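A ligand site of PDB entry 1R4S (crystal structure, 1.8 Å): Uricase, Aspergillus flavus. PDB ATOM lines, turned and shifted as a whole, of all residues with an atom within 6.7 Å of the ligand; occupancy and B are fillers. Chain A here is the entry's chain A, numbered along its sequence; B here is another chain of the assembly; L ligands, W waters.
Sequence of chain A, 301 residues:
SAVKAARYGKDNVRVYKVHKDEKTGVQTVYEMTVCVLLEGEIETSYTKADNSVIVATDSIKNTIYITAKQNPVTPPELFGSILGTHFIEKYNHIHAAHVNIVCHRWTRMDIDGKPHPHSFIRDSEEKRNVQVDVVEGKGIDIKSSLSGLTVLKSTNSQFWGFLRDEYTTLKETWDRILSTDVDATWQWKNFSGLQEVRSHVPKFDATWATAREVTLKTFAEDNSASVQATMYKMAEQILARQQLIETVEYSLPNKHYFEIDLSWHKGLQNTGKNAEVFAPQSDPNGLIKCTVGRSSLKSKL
An oxygen (O2) of the ligand is in hydrogen-bond range of the side-chain amide nitrogen (NE2) of Gln 228 (2.9 Å).
The backbone NH (N) of Thr 57 of chain B sits at hydrogen-bond distance from an oxygen (O3) of the ligand, at 3.2 Å.
O1 of the ligand is in hydrogen-bond range of NH2 of Arg 176 (2.9 Å).
A nitrogen (N3) of the ligand is in hydrogen-bond range of the side-chain hydroxyl (OG1) of Thr 57 of chain B.
The backbone NH (N) of Val 227 sits at hydrogen-bond distance from an oxygen (O1) of the ligand, 2.9 Å away.
The backbone NH (N) of Asp 58 of chain B sits at hydrogen-bond distance from an oxygen (O3) of the ligand (2.9 Å).
N2 of the ligand sits close to ND2 of Asn 254 (3.3 Å).
O of Asn 254 is in hydrogen-bond range of NE2 of His 256 (3.5 Å).
The backbone carbonyl oxygen (O) of Ser 226 lies within hydrogen-bond range of the side-chain hydroxyl (OG) of Ser 224.
The guanidinium group (NE) of Arg 176 is in hydrogen-bond range of the side-chain hydroxyl (OG) of Ser 157, 2.9 Å away.
The side-chain hydroxyl of Thr 57 of chain B sits at hydrogen-bond distance from the side-chain amino group of Lys 10 of chain B (3.0 Å).
The backbone NH (N) of Gln 228 sits close to the side-chain hydroxyl (OG) of Ser 226, 3.4 Å away.
OH of Tyr 8 of chain B sits at hydrogen-bond distance from O of Val 55 of chain B, 2.6 Å away.
N of Asn 254 lies within hydrogen-bond range of O of Gly 286 (2.8 Å).
Water W2 lies within hydrogen-bond range of the side-chain hydroxyl (OG1) of Thr 57 of chain B (2.7 Å), the side-chain amide nitrogen (ND2) of Asn 254 (2.9 Å) and a nitrogen (N3) of the ligand (3.4 Å).
Phe 159 touches the ligand.
CD2 of Leu 170 touches O3 of the ligand, 3.4 Å away.
CA of Ser 226 touches O1 of the ligand, 3.5 Å away.
Tyr 8 of chain B touches the ligand.
CG2 of Ile 54 of chain B touches O2 of the ligand (3.6 Å).
Ala 56 of chain B touches the ligand (CB to O3, 3.5 Å).
Within 4 Å of the ligand: Phe 159, Leu 170, Arg 176, Ser 226, Val 227, Gln 228, Asn 254, Tyr 8 of chain B, Ile 54 of chain B, Ala 56 of chain B, Thr 57 of chain B and Asp 58 of chain B.
The nearest printed residue that does not touch the ligand is His 256 (4.3 Å).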
ATOM      1  N   SER A 157      -8.252  18.751 -17.840  1.00  0.00           N
ATOM      2  CA  SER A 157      -8.805  20.066 -17.561  1.00  0.00           C
ATOM      3  C   SER A 157     -10.250  19.957 -18.069  1.00  0.00           C
ATOM      4  O   SER A 157     -10.502  19.356 -19.107  1.00  0.00           O
ATOM      5  CB  SER A 157      -8.035  21.206 -18.276  1.00  0.00           C
ATOM      6  OG  SER A 157      -8.820  22.403 -18.244  1.00  0.00           O
ATOM      7  N   GLN A 158     -11.194  20.428 -17.263  1.00  0.00           N
ATOM      8  CA  GLN A 158     -12.616  20.364 -17.567  1.00  0.00           C
ATOM      9  C   GLN A 158     -13.208  21.739 -17.326  1.00  0.00           C
ATOM     10  O   GLN A 158     -12.633  22.585 -16.636  1.00  0.00           O
ATOM     11  CB  GLN A 158     -13.301  19.373 -16.582  1.00  0.00           C
ATOM     12  CG  GLN A 158     -12.530  18.030 -16.460  1.00  0.00           C
ATOM     13  CD  GLN A 158     -13.311  16.963 -15.693  1.00  0.00           C
ATOM     14  OE1 GLN A 158     -14.364  17.225 -15.115  1.00  0.00           O
ATOM     15  NE2 GLN A 158     -12.756  15.766 -15.639  1.00  0.00           N
ATOM     16  N   PHE A 159     -14.368  21.956 -17.927  1.00  0.00           N
ATOM     17  CA  PHE A 159     -15.137  23.160 -17.670  1.00  0.00           C
ATOM     18  C   PHE A 159     -16.604  22.921 -17.987  1.00  0.00           C
ATOM     19  O   PHE A 159     -17.031  23.010 -19.141  1.00  0.00           O
ATOM     20  CB  PHE A 159     -14.572  24.404 -18.400  1.00  0.00           C
ATOM     21  CG  PHE A 159     -15.174  25.700 -17.908  1.00  0.00           C
ATOM     22  CD1 PHE A 159     -15.002  26.100 -16.580  1.00  0.00           C
ATOM     23  CD2 PHE A 159     -15.944  26.488 -18.743  1.00  0.00           C
ATOM     24  CE1 PHE A 159     -15.570  27.291 -16.108  1.00  0.00           C
ATOM     25  CE2 PHE A 159     -16.540  27.672 -18.283  1.00  0.00           C
ATOM     26  CZ  PHE A 159     -16.352  28.067 -16.956  1.00  0.00           C
ATOM     27  N   PHE A 162     -21.297  25.714 -15.684  1.00  0.00           N
ATOM     28  CA  PHE A 162     -21.346  27.162 -15.596  1.00  0.00           C
ATOM     29  C   PHE A 162     -22.756  27.678 -15.927  1.00  0.00           C
ATOM     30  O   PHE A 162     -23.549  26.950 -16.528  1.00  0.00           O
ATOM     31  CB  PHE A 162     -20.311  27.812 -16.561  1.00  0.00           C
ATOM     32  CG  PHE A 162     -20.296  27.212 -17.944  1.00  0.00           C
ATOM     33  CD1 PHE A 162     -19.457  26.152 -18.247  1.00  0.00           C
ATOM     34  CD2 PHE A 162     -21.093  27.746 -18.978  1.00  0.00           C
ATOM     35  CE1 PHE A 162     -19.427  25.588 -19.507  1.00  0.00           C
ATOM     36  CE2 PHE A 162     -21.058  27.185 -20.260  1.00  0.00           C
ATOM     37  CZ  PHE A 162     -20.221  26.108 -20.523  1.00  0.00           C
ATOM     38  N   LEU A 170     -21.363  28.533 -25.415  1.00  0.00           N
ATOM     39  CA  LEU A 170     -20.241  27.645 -25.094  1.00  0.00           C
ATOM     40  C   LEU A 170     -20.735  26.270 -24.669  1.00  0.00           C
ATOM     41  O   LEU A 170     -21.638  26.157 -23.845  1.00  0.00           O
ATOM     42  CB  LEU A 170     -19.413  28.291 -23.967  1.00  0.00           C
ATOM     43  CG  LEU A 170     -18.199  27.476 -23.406  1.00  0.00           C
ATOM     44  CD1 LEU A 170     -17.066  27.352 -24.438  1.00  0.00           C
ATOM     45  CD2 LEU A 170     -17.666  28.073 -22.116  1.00  0.00           C
ATOM     46  N   ARG A 176     -10.253  19.173 -22.042  1.00  0.00           N
ATOM     47  CA  ARG A 176      -9.792  20.263 -22.924  1.00  0.00           C
ATOM     48  C   ARG A 176      -8.334  20.564 -22.665  1.00  0.00           C
ATOM     49  O   ARG A 176      -7.722  20.073 -21.711  1.00  0.00           O
ATOM     50  CB  ARG A 176     -10.631  21.532 -22.687  1.00  0.00           C
ATOM     51  CG  ARG A 176     -10.411  22.120 -21.256  1.00  0.00           C
ATOM     52  CD  ARG A 176     -11.113  23.464 -21.069  1.00  0.00           C
ATOM     53  NE  ARG A 176     -10.753  24.011 -19.743  1.00  0.00           N
ATOM     54  CZ  ARG A 176     -11.125  25.187 -19.288  1.00  0.00           C
ATOM     55  NH1 ARG A 176     -11.966  25.958 -20.002  1.00  0.00           N
ATOM     56  NH2 ARG A 176     -10.657  25.580 -18.092  1.00  0.00           N
ATOM     57  N   LEU A 178      -5.481  23.169 -21.516  1.00  0.00           N
ATOM     58  CA  LEU A 178      -5.431  24.354 -20.654  1.00  0.00           C
ATOM     59  C   LEU A 178      -4.019  24.935 -20.840  1.00  0.00           C
ATOM     60  O   LEU A 178      -3.028  24.238 -20.642  1.00  0.00           O
ATOM     61  CB  LEU A 178      -5.702  23.997 -19.186  1.00  0.00           C
ATOM     62  CG  LEU A 178      -5.582  25.158 -18.178  1.00  0.00           C
ATOM     63  CD1 LEU A 178      -6.525  26.261 -18.573  1.00  0.00           C
ATOM     64  CD2 LEU A 178      -5.916  24.715 -16.725  1.00  0.00           C
ATOM     65  N   SER A 224      -8.196  19.738 -13.260  1.00  0.00           N
ATOM     66  CA  SER A 224      -8.792  21.047 -13.115  1.00  0.00           C
ATOM     67  C   SER A 224     -10.273  21.220 -13.429  1.00  0.00           C
ATOM     68  O   SER A 224     -10.727  20.962 -14.545  1.00  0.00           O
ATOM     69  CB  SER A 224      -7.902  22.082 -13.854  1.00  0.00           C
ATOM     70  OG  SER A 224      -8.530  23.345 -13.837  1.00  0.00           O
ATOM     71  N   ALA A 225     -11.006  21.749 -12.471  1.00  0.00           N
ATOM     72  CA  ALA A 225     -12.431  21.994 -12.631  1.00  0.00           C
ATOM     73  C   ALA A 225     -12.644  23.358 -13.311  1.00  0.00           C
ATOM     74  O   ALA A 225     -13.717  23.655 -13.838  1.00  0.00           O
ATOM     75  CB  ALA A 225     -13.095  21.999 -11.246  1.00  0.00           C
ATOM     76  N   SER A 226     -11.617  24.212 -13.248  1.00  0.00           N
ATOM     77  CA  SER A 226     -11.665  25.557 -13.831  1.00  0.00           C
ATOM     78  C   SER A 226     -10.333  26.227 -13.507  1.00  0.00           C
ATOM     79  O   SER A 226      -9.593  25.741 -12.632  1.00  0.00           O
ATOM     80  CB  SER A 226     -12.820  26.413 -13.247  1.00  0.00           C
ATOM     81  OG  SER A 226     -12.577  26.736 -11.872  1.00  0.00           O
ATOM     82  N   VAL A 227     -10.026  27.323 -14.200  1.00  0.00           N
ATOM     83  CA  VAL A 227      -8.803  28.047 -13.864  1.00  0.00           C
ATOM     84  C   VAL A 227      -8.956  28.573 -12.431  1.00  0.00           C
ATOM     85  O   VAL A 227      -7.994  28.555 -11.653  1.00  0.00           O
ATOM     86  CB  VAL A 227      -8.574  29.235 -14.865  1.00  0.00           C
ATOM     87  CG1 VAL A 227      -7.390  30.109 -14.421  1.00  0.00           C
ATOM     88  CG2 VAL A 227      -8.306  28.629 -16.274  1.00  0.00           C
ATOM     89  N   GLN A 228     -10.158  29.052 -12.097  1.00  0.00           N
ATOM     90  CA  GLN A 228     -10.435  29.611 -10.769  1.00  0.00           C
ATOM     91  C   GLN A 228     -10.043  28.622  -9.660  1.00  0.00           C
ATOM     92  O   GLN A 228      -9.360  28.973  -8.659  1.00  0.00           O
ATOM     93  CB  GLN A 228     -11.909  29.973 -10.667  1.00  0.00           C
ATOM     94  CG  GLN A 228     -12.335  31.279 -11.407  1.00  0.00           C
ATOM     95  CD  GLN A 228     -12.751  31.023 -12.874  1.00  0.00           C
ATOM     96  OE1 GLN A 228     -12.325  30.043 -13.515  1.00  0.00           O
ATOM     97  NE2 GLN A 228     -13.584  31.910 -13.402  1.00  0.00           N
ATOM     98  N   ASN A 254      -6.511  32.712 -20.002  1.00  0.00           N
ATOM     99  CA  ASN A 254      -6.894  31.386 -20.450  1.00  0.00           C
ATOM    100  C   ASN A 254      -6.659  31.430 -21.965  1.00  0.00           C
ATOM    101  O   ASN A 254      -7.414  32.092 -22.661  1.00  0.00           O
ATOM    102  CB  ASN A 254      -8.370  31.123 -20.095  1.00  0.00           C
ATOM    103  CG  ASN A 254      -8.804  29.672 -20.389  1.00  0.00           C
ATOM    104  OD1 ASN A 254      -8.006  28.844 -20.842  1.00  0.00           O
ATOM    105  ND2 ASN A 254     -10.074  29.378 -20.180  1.00  0.00           N
ATOM    106  N   HIS A 256      -6.886  30.154 -25.360  1.00  0.00           N
ATOM    107  CA  HIS A 256      -7.732  29.125 -25.973  1.00  0.00           C
ATOM    108  C   HIS A 256      -7.150  28.345 -27.132  1.00  0.00           C
ATOM    109  O   HIS A 256      -6.531  28.923 -28.008  1.00  0.00           O
ATOM    110  CB  HIS A 256      -9.069  29.749 -26.371  1.00  0.00           C
ATOM    111  CG  HIS A 256      -9.712  30.513 -25.260  1.00  0.00           C
ATOM    112  ND1 HIS A 256     -10.128  29.919 -24.086  1.00  0.00           N
ATOM    113  CD2 HIS A 256      -9.997  31.835 -25.131  1.00  0.00           C
ATOM    114  CE1 HIS A 256     -10.672  30.826 -23.294  1.00  0.00           C
ATOM    115  NE2 HIS A 256     -10.630  32.006 -23.921  1.00  0.00           N
ATOM    116  N   GLY A 286      -9.577  34.570 -21.973  1.00  0.00           N
ATOM    117  CA  GLY A 286     -10.146  34.744 -20.653  1.00  0.00           C
ATOM    118  C   GLY A 286      -9.028  35.358 -19.791  1.00  0.00           C
ATOM    119  O   GLY A 286      -7.835  35.210 -20.095  1.00  0.00           O
ATOM    120  N   ILE A 288      -8.348  35.646 -15.592  1.00  0.00           N
ATOM    121  CA  ILE A 288      -8.883  35.247 -14.294  1.00  0.00           C
ATOM    122  C   ILE A 288      -7.894  35.662 -13.190  1.00  0.00           C
ATOM    123  O   ILE A 288      -6.703  35.371 -13.300  1.00  0.00           O
ATOM    124  CB  ILE A 288      -9.061  33.671 -14.242  1.00  0.00           C
ATOM    125  CG1 ILE A 288      -9.958  33.151 -15.442  1.00  0.00           C
ATOM    126  CG2 ILE A 288      -9.784  33.294 -12.926  1.00  0.00           C
ATOM    127  CD1 ILE A 288      -9.194  32.582 -16.592  1.00  0.00           C
ATOM    128  N   TYR B   8     -12.809  38.385 -12.884  1.00  0.00           N
ATOM    129  CA  TYR B   8     -12.498  37.532 -14.035  1.00  0.00           C
ATOM    130  C   TYR B   8     -13.330  38.039 -15.226  1.00  0.00           C
ATOM    131  O   TYR B   8     -14.322  38.752 -15.072  1.00  0.00           O
ATOM    132  CB  TYR B   8     -12.776  36.053 -13.715  1.00  0.00           C
ATOM    133  CG  TYR B   8     -14.217  35.700 -13.880  1.00  0.00           C
ATOM    134  CD1 TYR B   8     -15.184  36.158 -12.966  1.00  0.00           C
ATOM    135  CD2 TYR B   8     -14.671  35.079 -15.055  1.00  0.00           C
ATOM    136  CE1 TYR B   8     -16.556  35.988 -13.213  1.00  0.00           C
ATOM    137  CE2 TYR B   8     -16.017  34.858 -15.285  1.00  0.00           C
ATOM    138  CZ  TYR B   8     -16.958  35.374 -14.376  1.00  0.00           C
ATOM    139  OH  TYR B   8     -18.295  35.163 -14.617  1.00  0.00           O
ATOM    140  N   GLY B   9     -12.882  37.691 -16.423  1.00  0.00           N
ATOM    141  CA  GLY B   9     -13.647  38.134 -17.586  1.00  0.00           C
ATOM    142  C   GLY B   9     -12.893  37.880 -18.873  1.00  0.00           C
ATOM    143  O   GLY B   9     -12.149  36.920 -18.976  1.00  0.00           O
ATOM    144  N   LYS B  10     -13.148  38.702 -19.887  1.00  0.00           N
ATOM    145  CA  LYS B  10     -12.548  38.463 -21.218  1.00  0.00           C
ATOM    146  C   LYS B  10     -11.724  39.679 -21.609  1.00  0.00           C
ATOM    147  O   LYS B  10     -12.173  40.826 -21.458  1.00  0.00           O
ATOM    148  CB  LYS B  10     -13.664  38.228 -22.267  1.00  0.00           C
ATOM    149  CG  LYS B  10     -13.170  37.550 -23.547  1.00  0.00           C
ATOM    150  CD  LYS B  10     -12.716  36.108 -23.245  1.00  0.00           C
ATOM    151  CE  LYS B  10     -13.292  35.066 -24.185  1.00  0.00           C
ATOM    152  NZ  LYS B  10     -13.024  33.657 -23.684  1.00  0.00           N
ATOM    153  N   ASN B  51     -18.990  25.975 -10.385  1.00  0.00           N
ATOM    154  CA  ASN B  51     -19.107  26.797 -11.586  1.00  0.00           C
ATOM    155  C   ASN B  51     -20.446  27.457 -11.801  1.00  0.00           C
ATOM    156  O   ASN B  51     -20.596  28.275 -12.706  1.00  0.00           O
ATOM    157  CB  ASN B  51     -18.642  26.007 -12.821  1.00  0.00           C
ATOM    158  CG  ASN B  51     -17.149  25.657 -12.757  1.00  0.00           C
ATOM    159  OD1 ASN B  51     -16.370  26.350 -12.071  1.00  0.00           O
ATOM    160  ND2 ASN B  51     -16.736  24.621 -13.490  1.00  0.00           N
ATOM    161  N   ILE B  54     -20.530  31.155 -12.264  1.00  0.00           N
ATOM    162  CA  ILE B  54     -19.712  31.756 -13.339  1.00  0.00           C
ATOM    163  C   ILE B  54     -20.471  32.035 -14.632  1.00  0.00           C
ATOM    164  O   ILE B  54     -21.061  31.132 -15.230  1.00  0.00           O
ATOM    165  CB  ILE B  54     -18.505  30.844 -13.685  1.00  0.00           C
ATOM    166  CG1 ILE B  54     -17.577  30.716 -12.463  1.00  0.00           C
ATOM    167  CG2 ILE B  54     -17.684  31.440 -14.885  1.00  0.00           C
ATOM    168  CD1 ILE B  54     -16.462  29.686 -12.700  1.00  0.00           C
ATOM    169  N   VAL B  55     -20.491  33.303 -15.016  1.00  0.00           N
ATOM    170  CA  VAL B  55     -20.980  33.721 -16.327  1.00  0.00           C
ATOM    171  C   VAL B  55     -19.711  33.455 -17.191  1.00  0.00           C
ATOM    172  O   VAL B  55     -18.669  34.083 -16.946  1.00  0.00           O
ATOM    173  CB  VAL B  55     -21.335  35.241 -16.340  1.00  0.00           C
ATOM    174  CG1 VAL B  55     -21.633  35.735 -17.767  1.00  0.00           C
ATOM    175  CG2 VAL B  55     -22.552  35.529 -15.411  1.00  0.00           C
ATOM    176  N   ALA B  56     -19.751  32.460 -18.074  1.00  0.00           N
ATOM    177  CA  ALA B  56     -18.557  32.059 -18.850  1.00  0.00           C
ATOM    178  C   ALA B  56     -17.940  33.251 -19.563  1.00  0.00           C
ATOM    179  O   ALA B  56     -18.677  34.130 -20.030  1.00  0.00           O
ATOM    180  CB  ALA B  56     -18.901  30.923 -19.846  1.00  0.00           C
ATOM    181  N   THR B  57     -16.602  33.293 -19.638  1.00  0.00           N
ATOM    182  CA  THR B  57     -15.944  34.411 -20.341  1.00  0.00           C
ATOM    183  C   THR B  57     -16.351  34.428 -21.832  1.00  0.00           C
ATOM    184  O   THR B  57     -16.537  35.482 -22.402  1.00  0.00           O
ATOM    185  CB  THR B  57     -14.406  34.430 -20.175  1.00  0.00           C
ATOM    186  OG1 THR B  57     -13.828  33.324 -20.865  1.00  0.00           O
ATOM    187  CG2 THR B  57     -14.000  34.387 -18.665  1.00  0.00           C
ATOM    188  N   ASP B  58     -16.618  33.247 -22.408  1.00  0.00           N
ATOM    189  CA  ASP B  58     -17.135  33.212 -23.786  1.00  0.00           C
ATOM    190  C   ASP B  58     -18.486  33.944 -23.902  1.00  0.00           C
ATOM    191  O   ASP B  58     -18.766  34.587 -24.906  1.00  0.00           O
ATOM    192  CB  ASP B  58     -17.302  31.762 -24.217  1.00  0.00           C
ATOM    193  CG  ASP B  58     -17.595  31.629 -25.699  1.00  0.00           C
ATOM    194  OD1 ASP B  58     -16.640  31.684 -26.492  1.00  0.00           O
ATOM    195  OD2 ASP B  58     -18.772  31.385 -26.048  1.00  0.00           O
ATOM    196  N   SER B  59     -19.348  33.826 -22.872  1.00  0.00           N
ATOM    197  CA  SER B  59     -20.640  34.532 -22.883  1.00  0.00           C
ATOM    198  C   SER B  59     -20.441  36.053 -22.758  1.00  0.00           C
ATOM    199  O   SER B  59     -21.219  36.853 -23.289  1.00  0.00           O
ATOM    200  CB  SER B  59     -21.543  34.011 -21.723  1.00  0.00           C
ATOM    201  OG  SER B  59     -21.625  32.583 -21.822  1.00  0.00           O
HETATM  202  N1  LIG L   1     -12.978  29.624 -16.382  1.00  0.00           N
HETATM  203  C1  LIG L   1     -12.386  28.594 -17.077  1.00  0.00           C
HETATM  204  O1  LIG L   1     -11.611  27.845 -16.517  1.00  0.00           O
HETATM  205  N2  LIG L   1     -12.698  28.434 -18.432  1.00  0.00           N
HETATM  206  C2  LIG L   1     -13.594  29.271 -18.929  1.00  0.00           C
HETATM  207  C3  LIG L   1     -14.211  30.297 -18.267  1.00  0.00           C
HETATM  208  C4  LIG L   1     -13.881  30.542 -16.860  1.00  0.00           C
HETATM  209  O2  LIG L   1     -14.342  31.437 -16.164  1.00  0.00           O
HETATM  210  N3  LIG L   1     -15.067  30.922 -19.080  1.00  0.00           N
HETATM  211  C5  LIG L   1     -15.045  30.337 -20.350  1.00  0.00           C
HETATM  212  N4  LIG L   1     -14.142  29.286 -20.348  1.00  0.00           N
HETATM  213  C6  LIG L   1     -13.716  28.315 -21.476  1.00  0.00           C
HETATM  214  O3  LIG L   1     -15.722  30.672 -21.286  1.00  0.00           O
HETATM  215  O   HOH W   1     -13.967  25.136 -22.361  1.00  0.00           O
HETATM  216  O   HOH W   2     -11.846  31.712 -19.871  1.00  0.00           O
